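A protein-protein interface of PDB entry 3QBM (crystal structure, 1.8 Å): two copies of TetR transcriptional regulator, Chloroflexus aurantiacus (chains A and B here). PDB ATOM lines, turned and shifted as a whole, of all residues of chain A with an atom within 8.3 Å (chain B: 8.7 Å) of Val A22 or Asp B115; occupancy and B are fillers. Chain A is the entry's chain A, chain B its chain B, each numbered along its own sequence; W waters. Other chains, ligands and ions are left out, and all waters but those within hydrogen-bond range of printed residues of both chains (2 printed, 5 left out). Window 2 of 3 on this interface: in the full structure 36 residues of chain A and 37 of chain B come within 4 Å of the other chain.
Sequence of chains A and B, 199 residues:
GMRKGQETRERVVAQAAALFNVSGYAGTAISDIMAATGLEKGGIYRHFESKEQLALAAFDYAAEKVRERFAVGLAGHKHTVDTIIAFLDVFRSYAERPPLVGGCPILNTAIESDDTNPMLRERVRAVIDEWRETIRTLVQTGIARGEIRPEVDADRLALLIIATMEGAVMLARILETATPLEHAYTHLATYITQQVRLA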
ATOM      1  N   ALA A  16      -8.511  27.002  -8.402  1.00  0.00           N
ATOM      2  CA  ALA A  16      -9.920  26.954  -7.963  1.00  0.00           C
ATOM      3  C   ALA A  16     -10.041  25.943  -6.826  1.00  0.00           C
ATOM      4  O   ALA A  16     -10.661  26.227  -5.800  1.00  0.00           O
ATOM      5  CB  ALA A  16     -10.831  26.566  -9.093  1.00  0.00           C
ATOM      6  N   ALA A  17      -9.410  24.784  -7.003  1.00  0.00           N
ATOM      7  CA  ALA A  17      -9.475  23.717  -5.990  1.00  0.00           C
ATOM      8  C   ALA A  17      -9.022  24.194  -4.632  1.00  0.00           C
ATOM      9  O   ALA A  17      -9.672  23.909  -3.618  1.00  0.00           O
ATOM     10  CB  ALA A  17      -8.662  22.453  -6.410  1.00  0.00           C
ATOM     11  N   ALA A  18      -7.919  24.930  -4.591  1.00  0.00           N
ATOM     12  CA  ALA A  18      -7.381  25.405  -3.310  1.00  0.00           C
ATOM     13  C   ALA A  18      -8.327  26.385  -2.663  1.00  0.00           C
ATOM     14  O   ALA A  18      -8.559  26.320  -1.458  1.00  0.00           O
ATOM     15  CB  ALA A  18      -5.987  26.024  -3.484  1.00  0.00           C
ATOM     16  N   LEU A  19      -8.932  27.287  -3.453  1.00  0.00           N
ATOM     17  CA  LEU A  19      -9.867  28.225  -2.877  1.00  0.00           C
ATOM     18  C   LEU A  19     -11.141  27.521  -2.373  1.00  0.00           C
ATOM     19  O   LEU A  19     -11.670  27.862  -1.309  1.00  0.00           O
ATOM     20  CB  LEU A  19     -10.264  29.304  -3.898  1.00  0.00           C
ATOM     21  CG  LEU A  19      -9.158  30.316  -4.253  1.00  0.00           C
ATOM     22  CD1 LEU A  19      -9.496  31.107  -5.539  1.00  0.00           C
ATOM     23  CD2 LEU A  19      -8.941  31.274  -3.097  1.00  0.00           C
ATOM     24  N   PHE A  20     -11.670  26.597  -3.176  1.00  0.00           N
ATOM     25  CA  PHE A  20     -12.913  25.915  -2.810  1.00  0.00           C
ATOM     26  C   PHE A  20     -12.694  25.072  -1.541  1.00  0.00           C
ATOM     27  O   PHE A  20     -13.603  24.882  -0.744  1.00  0.00           O
ATOM     28  CB  PHE A  20     -13.391  24.954  -3.905  1.00  0.00           C
ATOM     29  CG  PHE A  20     -13.867  25.599  -5.161  1.00  0.00           C
ATOM     30  CD1 PHE A  20     -14.749  26.659  -5.144  1.00  0.00           C
ATOM     31  CD2 PHE A  20     -13.524  25.053  -6.396  1.00  0.00           C
ATOM     32  CE1 PHE A  20     -15.219  27.201  -6.313  1.00  0.00           C
ATOM     33  CE2 PHE A  20     -14.006  25.592  -7.559  1.00  0.00           C
ATOM     34  CZ  PHE A  20     -14.835  26.656  -7.528  1.00  0.00           C
ATOM     35  N   ASN A  21     -11.491  24.550  -1.381  1.00  0.00           N
ATOM     36  CA  ASN A  21     -11.200  23.694  -0.230  1.00  0.00           C
ATOM     37  C   ASN A  21     -11.290  24.420   1.118  1.00  0.00           C
ATOM     38  O   ASN A  21     -11.623  23.804   2.163  1.00  0.00           O
ATOM     39  CB  ASN A  21      -9.829  23.051  -0.365  1.00  0.00           C
ATOM     40  CG  ASN A  21      -9.719  21.788   0.433  1.00  0.00           C
ATOM     41  OD1 ASN A  21     -10.675  21.027   0.491  1.00  0.00           O
ATOM     42  ND2 ASN A  21      -8.543  21.541   1.042  1.00  0.00           N
ATOM     43  N   VAL A  22     -11.024  25.717   1.073  1.00  0.00           N
ATOM     44  CA  VAL A  22     -11.082  26.582   2.239  1.00  0.00           C
ATOM     45  C   VAL A  22     -12.431  27.241   2.454  1.00  0.00           C
ATOM     46  O   VAL A  22     -13.008  27.137   3.551  1.00  0.00           O
ATOM     47  CB  VAL A  22      -9.982  27.680   2.132  1.00  0.00           C
ATOM     48  CG1 VAL A  22     -10.203  28.778   3.174  1.00  0.00           C
ATOM     49  CG2 VAL A  22      -8.622  27.045   2.215  1.00  0.00           C
ATOM     50  N   SER A  23     -12.939  27.923   1.420  1.00  0.00           N
ATOM     51  CA  SER A  23     -14.123  28.746   1.544  1.00  0.00           C
ATOM     52  C   SER A  23     -15.379  28.099   0.991  1.00  0.00           C
ATOM     53  O   SER A  23     -16.460  28.685   1.054  1.00  0.00           O
ATOM     54  CB  SER A  23     -13.880  30.102   0.845  1.00  0.00           C
ATOM     55  OG  SER A  23     -12.815  30.756   1.479  1.00  0.00           O
ATOM     56  N   GLY A  24     -15.235  26.899   0.451  1.00  0.00           N
ATOM     57  CA  GLY A  24     -16.334  26.172  -0.103  1.00  0.00           C
ATOM     58  C   GLY A  24     -16.636  26.614  -1.526  1.00  0.00           C
ATOM     59  O   GLY A  24     -16.061  27.575  -2.051  1.00  0.00           O
ATOM     60  N   TYR A  25     -17.577  25.910  -2.129  1.00  0.00           N
ATOM     61  CA  TYR A  25     -18.028  26.191  -3.491  1.00  0.00           C
ATOM     62  C   TYR A  25     -18.918  27.448  -3.501  1.00  0.00           C
ATOM     63  O   TYR A  25     -18.637  28.409  -4.213  1.00  0.00           O
ATOM     64  CB  TYR A  25     -18.695  24.930  -4.077  1.00  0.00           C
ATOM     65  CG  TYR A  25     -17.722  23.731  -4.118  1.00  0.00           C
ATOM     66  CD1 TYR A  25     -16.871  23.537  -5.202  1.00  0.00           C
ATOM     67  CD2 TYR A  25     -17.629  22.817  -3.066  1.00  0.00           C
ATOM     68  CE1 TYR A  25     -15.951  22.477  -5.242  1.00  0.00           C
ATOM     69  CE2 TYR A  25     -16.686  21.768  -3.102  1.00  0.00           C
ATOM     70  CZ  TYR A  25     -15.863  21.618  -4.206  1.00  0.00           C
ATOM     71  OH  TYR A  25     -14.934  20.608  -4.321  1.00  0.00           O
ATOM     72  N   GLY A  27     -19.136  29.754  -1.242  1.00  0.00           N
ATOM     73  CA  GLY A  27     -18.400  30.857  -0.626  1.00  0.00           C
ATOM     74  C   GLY A  27     -17.178  31.368  -1.370  1.00  0.00           C
ATOM     75  O   GLY A  27     -16.529  32.280  -0.889  1.00  0.00           O
ATOM     76  N   THR A  28     -16.841  30.763  -2.508  1.00  0.00           N
ATOM     77  CA  THR A  28     -15.706  31.171  -3.336  1.00  0.00           C
ATOM     78  C   THR A  28     -16.321  31.914  -4.536  1.00  0.00           C
ATOM     79  O   THR A  28     -17.038  31.295  -5.328  1.00  0.00           O
ATOM     80  CB  THR A  28     -14.866  29.950  -3.804  1.00  0.00           C
ATOM     81  OG1 THR A  28     -14.189  29.348  -2.682  1.00  0.00           O
ATOM     82  CG2 THR A  28     -13.805  30.332  -4.861  1.00  0.00           C
ATOM     83  N   PRO A  98      -1.857  18.704   4.629  1.00  0.00           N
ATOM     84  CA  PRO A  98      -3.057  18.189   4.012  1.00  0.00           C
ATOM     85  C   PRO A  98      -2.854  18.027   2.498  1.00  0.00           C
ATOM     86  O   PRO A  98      -1.838  18.521   1.982  1.00  0.00           O
ATOM     87  CB  PRO A  98      -4.115  19.258   4.371  1.00  0.00           C
ATOM     88  CG  PRO A  98      -3.326  20.516   4.546  1.00  0.00           C
ATOM     89  CD  PRO A  98      -2.012  20.096   5.088  1.00  0.00           C
ATOM     90  N   LEU A 100      -4.302  19.296   0.002  1.00  0.00           N
ATOM     91  CA  LEU A 100      -4.090  20.677  -0.419  1.00  0.00           C
ATOM     92  C   LEU A 100      -4.507  21.651   0.702  1.00  0.00           C
ATOM     93  O   LEU A 100      -5.063  21.235   1.724  1.00  0.00           O
ATOM     94  CB  LEU A 100      -4.746  20.925  -1.758  1.00  0.00           C
ATOM     95  CG  LEU A 100      -6.240  20.897  -1.931  1.00  0.00           C
ATOM     96  CD1 LEU A 100      -6.796  22.143  -1.305  1.00  0.00           C
ATOM     97  CD2 LEU A 100      -6.611  20.883  -3.430  1.00  0.00           C
ATOM     98  N   VAL A 101      -4.206  22.926   0.515  1.00  0.00           N
ATOM     99  CA  VAL A 101      -4.470  23.935   1.539  1.00  0.00           C
ATOM    100  C   VAL A 101      -5.935  23.871   1.993  1.00  0.00           C
ATOM    101  O   VAL A 101      -6.812  23.795   1.195  1.00  0.00           O
ATOM    102  CB  VAL A 101      -4.185  25.327   1.015  1.00  0.00           C
ATOM    103  CG1 VAL A 101      -5.297  25.750   0.047  1.00  0.00           C
ATOM    104  CG2 VAL A 101      -4.017  26.324   2.185  1.00  0.00           C
ATOM    105  N   GLY A 102      -6.167  23.834   3.286  1.00  0.00           N
ATOM    106  CA  GLY A 102      -7.527  23.757   3.824  1.00  0.00           C
ATOM    107  C   GLY A 102      -8.038  22.393   4.241  1.00  0.00           C
ATOM    108  O   GLY A 102      -9.173  22.288   4.666  1.00  0.00           O
ATOM    109  N   GLY A 103      -7.221  21.347   4.174  1.00  0.00           N
ATOM    110  CA  GLY A 103      -7.601  20.041   4.688  1.00  0.00           C
ATOM    111  C   GLY A 103      -7.927  18.994   3.640  1.00  0.00           C
ATOM    112  O   GLY A 103      -7.497  19.104   2.480  1.00  0.00           O
ATOM    113  N   CYS A 104      -8.633  17.943   4.050  1.00  0.00           N
ATOM    114  CA  CYS A 104      -9.053  16.890   3.109  1.00  0.00           C
ATOM    115  C   CYS A 104     -10.186  17.372   2.213  1.00  0.00           C
ATOM    116  O   CYS A 104     -11.264  17.693   2.717  1.00  0.00           O
ATOM    117  CB  CYS A 104      -9.498  15.599   3.835  1.00  0.00           C
ATOM    118  SG  CYS A 104     -10.059  14.334   2.734  1.00  0.00           S
ATOM    119  N   PRO A 105      -9.976  17.383   0.883  1.00  0.00           N
ATOM    120  CA  PRO A 105     -11.060  17.859   0.000  1.00  0.00           C
ATOM    121  C   PRO A 105     -12.227  16.898  -0.128  1.00  0.00           C
ATOM    122  O   PRO A 105     -13.344  17.308  -0.518  1.00  0.00           O
ATOM    123  CB  PRO A 105     -10.355  18.038  -1.343  1.00  0.00           C
ATOM    124  CG  PRO A 105      -9.285  16.998  -1.316  1.00  0.00           C
ATOM    125  CD  PRO A 105      -8.791  16.964   0.115  1.00  0.00           C
ATOM    126  N   ASN A 108     -14.118  17.829   3.121  1.00  0.00           N
ATOM    127  CA  ASN A 108     -14.664  19.163   2.970  1.00  0.00           C
ATOM    128  C   ASN A 108     -15.814  19.217   1.926  1.00  0.00           C
ATOM    129  O   ASN A 108     -16.840  19.883   2.148  1.00  0.00           O
ATOM    130  CB  ASN A 108     -13.565  20.148   2.593  1.00  0.00           C
ATOM    131  CG  ASN A 108     -12.554  20.384   3.706  1.00  0.00           C
ATOM    132  OD1 ASN A 108     -12.746  19.980   4.864  1.00  0.00           O
ATOM    133  ND2 ASN A 108     -11.442  21.025   3.342  1.00  0.00           N
ATOM    134  N   GLU A 112     -20.283  19.923   2.266  1.00  0.00           N
ATOM    135  CA  GLU A 112     -21.022  20.887   1.450  1.00  0.00           C
ATOM    136  C   GLU A 112     -22.014  20.240   0.497  1.00  0.00           C
ATOM    137  O   GLU A 112     -23.174  20.683   0.388  1.00  0.00           O
ATOM    138  CB  GLU A 112     -20.081  21.766   0.629  1.00  0.00           C
ATOM    139  CG  GLU A 112     -20.877  22.884  -0.116  1.00  0.00           C
ATOM    140  CD  GLU A 112     -20.050  24.095  -0.522  1.00  0.00           C
ATOM    141  OE1 GLU A 112     -18.814  24.008  -0.497  1.00  0.00           O
ATOM    142  OE2 GLU A 112     -20.655  25.152  -0.832  1.00  0.00           O
ATOM    143  N   ARG A 173      -8.095  19.716  12.898  1.00  0.00           N
ATOM    144  CA  ARG A 173      -8.099  21.063  12.350  1.00  0.00           C
ATOM    145  C   ARG A 173      -8.830  22.019  13.262  1.00  0.00           C
ATOM    146  O   ARG A 173      -8.337  23.115  13.549  1.00  0.00           O
ATOM    147  CB  ARG A 173      -8.657  21.132  10.938  1.00  0.00           C
ATOM    148  CG  ARG A 173      -7.791  20.553   9.848  1.00  0.00           C
ATOM    149  CD  ARG A 173      -8.238  21.045   8.418  1.00  0.00           C
ATOM    150  NE  ARG A 173      -7.769  22.370   8.050  1.00  0.00           N
ATOM    151  CZ  ARG A 173      -6.513  22.641   7.702  1.00  0.00           C
ATOM    152  NH1 ARG A 173      -5.585  21.688   7.732  1.00  0.00           N
ATOM    153  NH2 ARG A 173      -6.150  23.866   7.377  1.00  0.00           N
ATOM    154  N   ILE A 174      -9.975  21.591  13.785  1.00  0.00           N
ATOM    155  CA  ILE A 174     -10.748  22.473  14.634  1.00  0.00           C
ATOM    156  C   ILE A 174     -10.109  22.709  16.027  1.00  0.00           C
ATOM    157  O   ILE A 174     -10.148  23.845  16.548  1.00  0.00           O
ATOM    158  CB  ILE A 174     -12.277  22.032  14.622  1.00  0.00           C
ATOM    159  CG1 ILE A 174     -13.200  23.225  14.852  1.00  0.00           C
ATOM    160  CG2 ILE A 174     -12.492  20.847  15.582  1.00  0.00           C
ATOM    161  CD1 ILE A 174     -13.222  24.299  13.712  1.00  0.00           C
ATOM    162  N   GLU A 176      -6.824  22.458  16.492  1.00  0.00           N
ATOM    163  CA  GLU A 176      -5.494  23.036  16.181  1.00  0.00           C
ATOM    164  C   GLU A 176      -4.367  22.237  16.853  1.00  0.00           C
ATOM    165  O   GLU A 176      -3.414  22.773  17.426  1.00  0.00           O
ATOM    166  CB  GLU A 176      -5.461  24.541  16.521  1.00  0.00           C
ATOM    167  CG  GLU A 176      -6.410  25.344  15.615  1.00  0.00           C
ATOM    168  CD  GLU A 176      -6.739  26.762  16.120  1.00  0.00           C
ATOM    169  OE1 GLU A 176      -5.938  27.325  16.890  1.00  0.00           O
ATOM    170  OE2 GLU A 176      -7.807  27.310  15.713  1.00  0.00           O
ATOM    171  N   ALA B  26     -21.805  31.128   4.293  1.00  0.00           N
ATOM    172  CA  ALA B  26     -21.566  31.842   3.043  1.00  0.00           C
ATOM    173  C   ALA B  26     -22.523  31.467   1.920  1.00  0.00           C
ATOM    174  O   ALA B  26     -22.887  32.315   1.112  1.00  0.00           O
ATOM    175  CB  ALA B  26     -20.112  31.623   2.578  1.00  0.00           C
ATOM    176  N   THR B 109     -20.299  22.865  10.747  1.00  0.00           N
ATOM    177  CA  THR B 109     -19.730  24.176  10.987  1.00  0.00           C
ATOM    178  C   THR B 109     -18.216  24.094  11.120  1.00  0.00           C
ATOM    179  O   THR B 109     -17.498  25.008  10.742  1.00  0.00           O
ATOM    180  CB  THR B 109     -20.359  24.858  12.235  1.00  0.00           C
ATOM    181  OG1 THR B 109     -21.781  24.913  12.078  1.00  0.00           O
ATOM    182  CG2 THR B 109     -19.852  26.250  12.404  1.00  0.00           C
ATOM    183  N   ALA B 110     -17.737  22.985  11.661  1.00  0.00           N
ATOM    184  CA  ALA B 110     -16.304  22.732  11.785  1.00  0.00           C
ATOM    185  C   ALA B 110     -15.598  22.856  10.425  1.00  0.00           C
ATOM    186  O   ALA B 110     -14.577  23.533  10.295  1.00  0.00           O
ATOM    187  CB  ALA B 110     -16.065  21.346  12.429  1.00  0.00           C
ATOM    188  N   ILE B 111     -16.159  22.214   9.408  1.00  0.00           N
ATOM    189  CA  ILE B 111     -15.562  22.207   8.076  1.00  0.00           C
ATOM    190  C   ILE B 111     -15.522  23.598   7.479  1.00  0.00           C
ATOM    191  O   ILE B 111     -14.498  24.001   6.911  1.00  0.00           O
ATOM    192  CB  ILE B 111     -16.276  21.210   7.115  1.00  0.00           C
ATOM    193  CG1 ILE B 111     -15.684  19.815   7.204  1.00  0.00           C
ATOM    194  CG2 ILE B 111     -16.040  21.592   5.640  1.00  0.00           C
ATOM    195  CD1 ILE B 111     -15.467  19.255   8.549  1.00  0.00           C
ATOM    196  N   GLU B 112     -16.615  24.348   7.632  1.00  0.00           N
ATOM    197  CA  GLU B 112     -16.666  25.700   7.102  1.00  0.00           C
ATOM    198  C   GLU B 112     -15.782  26.679   7.834  1.00  0.00           C
ATOM    199  O   GLU B 112     -14.982  27.358   7.217  1.00  0.00           O
ATOM    200  CB  GLU B 112     -18.099  26.217   7.078  1.00  0.00           C
ATOM    201  CG  GLU B 112     -18.159  27.657   6.507  1.00  0.00           C
ATOM    202  CD  GLU B 112     -19.508  28.000   5.974  1.00  0.00           C
ATOM    203  OE1 GLU B 112     -20.475  27.383   6.453  1.00  0.00           O
ATOM    204  OE2 GLU B 112     -19.581  28.859   5.068  1.00  0.00           O
ATOM    205  N   SER B 113     -15.909  26.715   9.154  1.00  0.00           N
ATOM    206  CA  SER B 113     -15.229  27.713   9.971  1.00  0.00           C
ATOM    207  C   SER B 113     -13.752  27.506  10.240  1.00  0.00           C
ATOM    208  O   SER B 113     -13.072  28.466  10.546  1.00  0.00           O
ATOM    209  CB  SER B 113     -15.940  27.835  11.324  1.00  0.00           C
ATOM    210  OG  SER B 113     -15.825  26.641  12.094  1.00  0.00           O
ATOM    211  N   ASP B 114     -13.250  26.273  10.149  1.00  0.00           N
ATOM    212  CA  ASP B 114     -11.868  26.005  10.578  1.00  0.00           C
ATOM    213  C   ASP B 114     -10.835  26.899   9.943  1.00  0.00           C
ATOM    214  O   ASP B 114      -9.886  27.300  10.601  1.00  0.00           O
ATOM    215  CB  ASP B 114     -11.499  24.525  10.495  1.00  0.00           C
ATOM    216  CG  ASP B 114     -11.687  23.909   9.112  1.00  0.00           C
ATOM    217  OD1 ASP B 114     -12.064  24.605   8.119  1.00  0.00           O
ATOM    218  OD2 ASP B 114     -11.453  22.685   9.018  1.00  0.00           O
ATOM    219  N   ASP B 115     -11.034  27.249   8.672  1.00  0.00           N
ATOM    220  CA  ASP B 115     -10.129  28.117   7.949  1.00  0.00           C
ATOM    221  C   ASP B 115     -10.734  29.456   7.514  1.00  0.00           C
ATOM    222  O   ASP B 115     -10.128  30.232   6.775  1.00  0.00           O
ATOM    223  CB  ASP B 115      -9.519  27.317   6.801  1.00  0.00           C
ATOM    224  CG  ASP B 115      -8.562  26.231   7.322  1.00  0.00           C
ATOM    225  OD1 ASP B 115      -7.656  26.588   8.110  1.00  0.00           O
ATOM    226  OD2 ASP B 115      -8.772  25.030   7.054  1.00  0.00           O
ATOM    227  N   THR B 116     -11.896  29.787   8.052  1.00  0.00           N
ATOM    228  CA  THR B 116     -12.572  31.008   7.637  1.00  0.00           C
ATOM    229  C   THR B 116     -13.088  31.915   8.750  1.00  0.00           C
ATOM    230  O   THR B 116     -13.170  33.093   8.518  1.00  0.00           O
ATOM    231  CB  THR B 116     -13.759  30.699   6.718  1.00  0.00           C
ATOM    232  OG1 THR B 116     -14.795  30.041   7.475  1.00  0.00           O
ATOM    233  CG2 THR B 116     -13.349  29.780   5.575  1.00  0.00           C
ATOM    234  N   ASN B 117     -13.421  31.402   9.942  1.00  0.00           N
ATOM    235  CA  ASN B 117     -14.191  32.204  10.910  1.00  0.00           C
ATOM    236  C   ASN B 117     -13.855  31.912  12.353  1.00  0.00           C
ATOM    237  O   ASN B 117     -14.313  30.911  12.897  1.00  0.00           O
ATOM    238  CB  ASN B 117     -15.709  32.021  10.685  1.00  0.00           C
ATOM    239  CG  ASN B 117     -16.536  33.122  11.340  1.00  0.00           C
ATOM    240  OD1 ASN B 117     -16.768  33.122  12.559  1.00  0.00           O
ATOM    241  ND2 ASN B 117     -16.971  34.114  10.519  1.00  0.00           N
ATOM    242  N   PRO B 118     -13.073  32.795  12.987  1.00  0.00           N
ATOM    243  CA  PRO B 118     -12.704  32.575  14.388  1.00  0.00           C
ATOM    244  C   PRO B 118     -13.851  32.402  15.377  1.00  0.00           C
ATOM    245  O   PRO B 118     -13.781  31.519  16.240  1.00  0.00           O
ATOM    246  CB  PRO B 118     -11.901  33.835  14.747  1.00  0.00           C
ATOM    247  CG  PRO B 118     -11.311  34.308  13.419  1.00  0.00           C
ATOM    248  CD  PRO B 118     -12.276  33.856  12.351  1.00  0.00           C
ATOM    249  N   ARG B 121     -15.469  28.998  14.823  1.00  0.00           N
ATOM    250  CA  ARG B 121     -14.477  28.025  15.310  1.00  0.00           C
ATOM    251  C   ARG B 121     -14.561  27.859  16.807  1.00  0.00           C
ATOM    252  O   ARG B 121     -14.566  26.731  17.320  1.00  0.00           O
ATOM    253  CB  ARG B 121     -13.038  28.478  15.032  1.00  0.00           C
ATOM    254  CG  ARG B 121     -12.537  28.173  13.705  1.00  0.00           C
ATOM    255  CD  ARG B 121     -11.008  28.101  13.722  1.00  0.00           C
ATOM    256  NE  ARG B 121     -10.314  29.366  14.004  1.00  0.00           N
ATOM    257  CZ  ARG B 121     -10.050  30.309  13.107  1.00  0.00           C
ATOM    258  NH1 ARG B 121     -10.488  30.197  11.844  1.00  0.00           N
ATOM    259  NH2 ARG B 121      -9.378  31.400  13.483  1.00  0.00           N
HETATM  260  O   HOH W   1     -17.333  29.767   3.393  1.00  0.00           O
HETATM  261  O   HOH W   2     -15.879  26.611   4.008  1.00  0.00           O
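The side-chain amide nitrogen of Asn A108 is in hydrogen-bond range of the backbone carbonyl oxygen of Gly A102 (2.9 Å).
The backbone carbonyl oxygen of Cys A104 lies close to the side-chain amide nitrogen of Asn A108.
The backbone carbonyl oxygen of Thr B109 lies within hydrogen-bond range of the side-chain hydroxyl of Ser B113, 2.7 Å away.
The side-chain hydroxyl of Thr B116 sits at hydrogen-bond distance from the backbone carbonyl oxygen of Glu B112 (2.7 Å).
The guanidinium group of Arg B121 lies close to the backbone carbonyl oxygen of Ser B113, at 3.4 Å.
The backbone carbonyl oxygen (O) of Asp B114 is in hydrogen-bond range of the guanidinium group (NH1) of Arg B121 (3.2 Å).
Asp B115 touches Val A22 (O to CG1, 3.9 Å).
Val A22 touches Thr B116.
CA of Gly A27 touches CB of Ala B26, at 3.7 Å.
OD2 of Asp B115 touches O of Gly A102 (3.7 Å).
Asn A108 touches Ile B111.
Ile A174 touches Ala B110 (CD1 to O, 3.8 Å).
Ser B113 touches Ile A174.
Ile A174 touches Asp B114 (CD1 to CB, 3.7 Å).
Ile A174 touches Arg B121 (CD1 to CG, 3.9 Å).
Water W1 lies within hydrogen-bond range of the backbone carbonyl oxygen of Ser A23 and the side-chain carboxylate of Glu B112.
Water W2 bridges the backbone carbonyl oxygen (O) of Val A22 (3.0 Å) and the backbone carbonyl oxygen (O) of Glu B112 (3.4 Å).
1 position is printed for both chains.
Of chain B, only Asp B115 and Thr B116 come within 4 Å of Val A22.
Gly A102 touches just one residue of chain B: Asp B115 (3.7 Å).
Of the printed residues of chain B, Asn A108 touches Ile B111 (3.7 Å).
Printed residues of chain A within 4 Å of Ala B26: Gly A27.
Of the printed residues of chain A, Ala B110 touches Ile A174 (3.8 Å).
Asp B114 touches just these residues of chain A: Arg A173 and Ile A174.
Asp B115 touches just these residues of chain A: Val A22, Gly A102 and Arg A173.
Printed residues of chain A within 4 Å of Thr B116: Val A22 (3.3 Å).
The nearest residue of chain A that does not touch Asp B115 is Gly A103 (4.9 Å).
Hydrophobic or aromatic side chains of chain A within 4 Å of the printed part of chain B: Val A22 and Ile A174.
Along chain A the printed residues that touch a printed residue of chain B span positions 22 to 176.
Of the 12 printed residues of chain B, 8 touch a printed residue of chain A.
OD2 of Asp B114 lies within salt-bridge range of NE of Arg A173 (3.8 Å).
NH2 of Arg A173 is in salt-bridge range of OD2 of Asp B115, 2.9 Å away.
NE of Arg B121 is in salt-bridge range of OE2 of Glu A176, at 3.7 Å.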
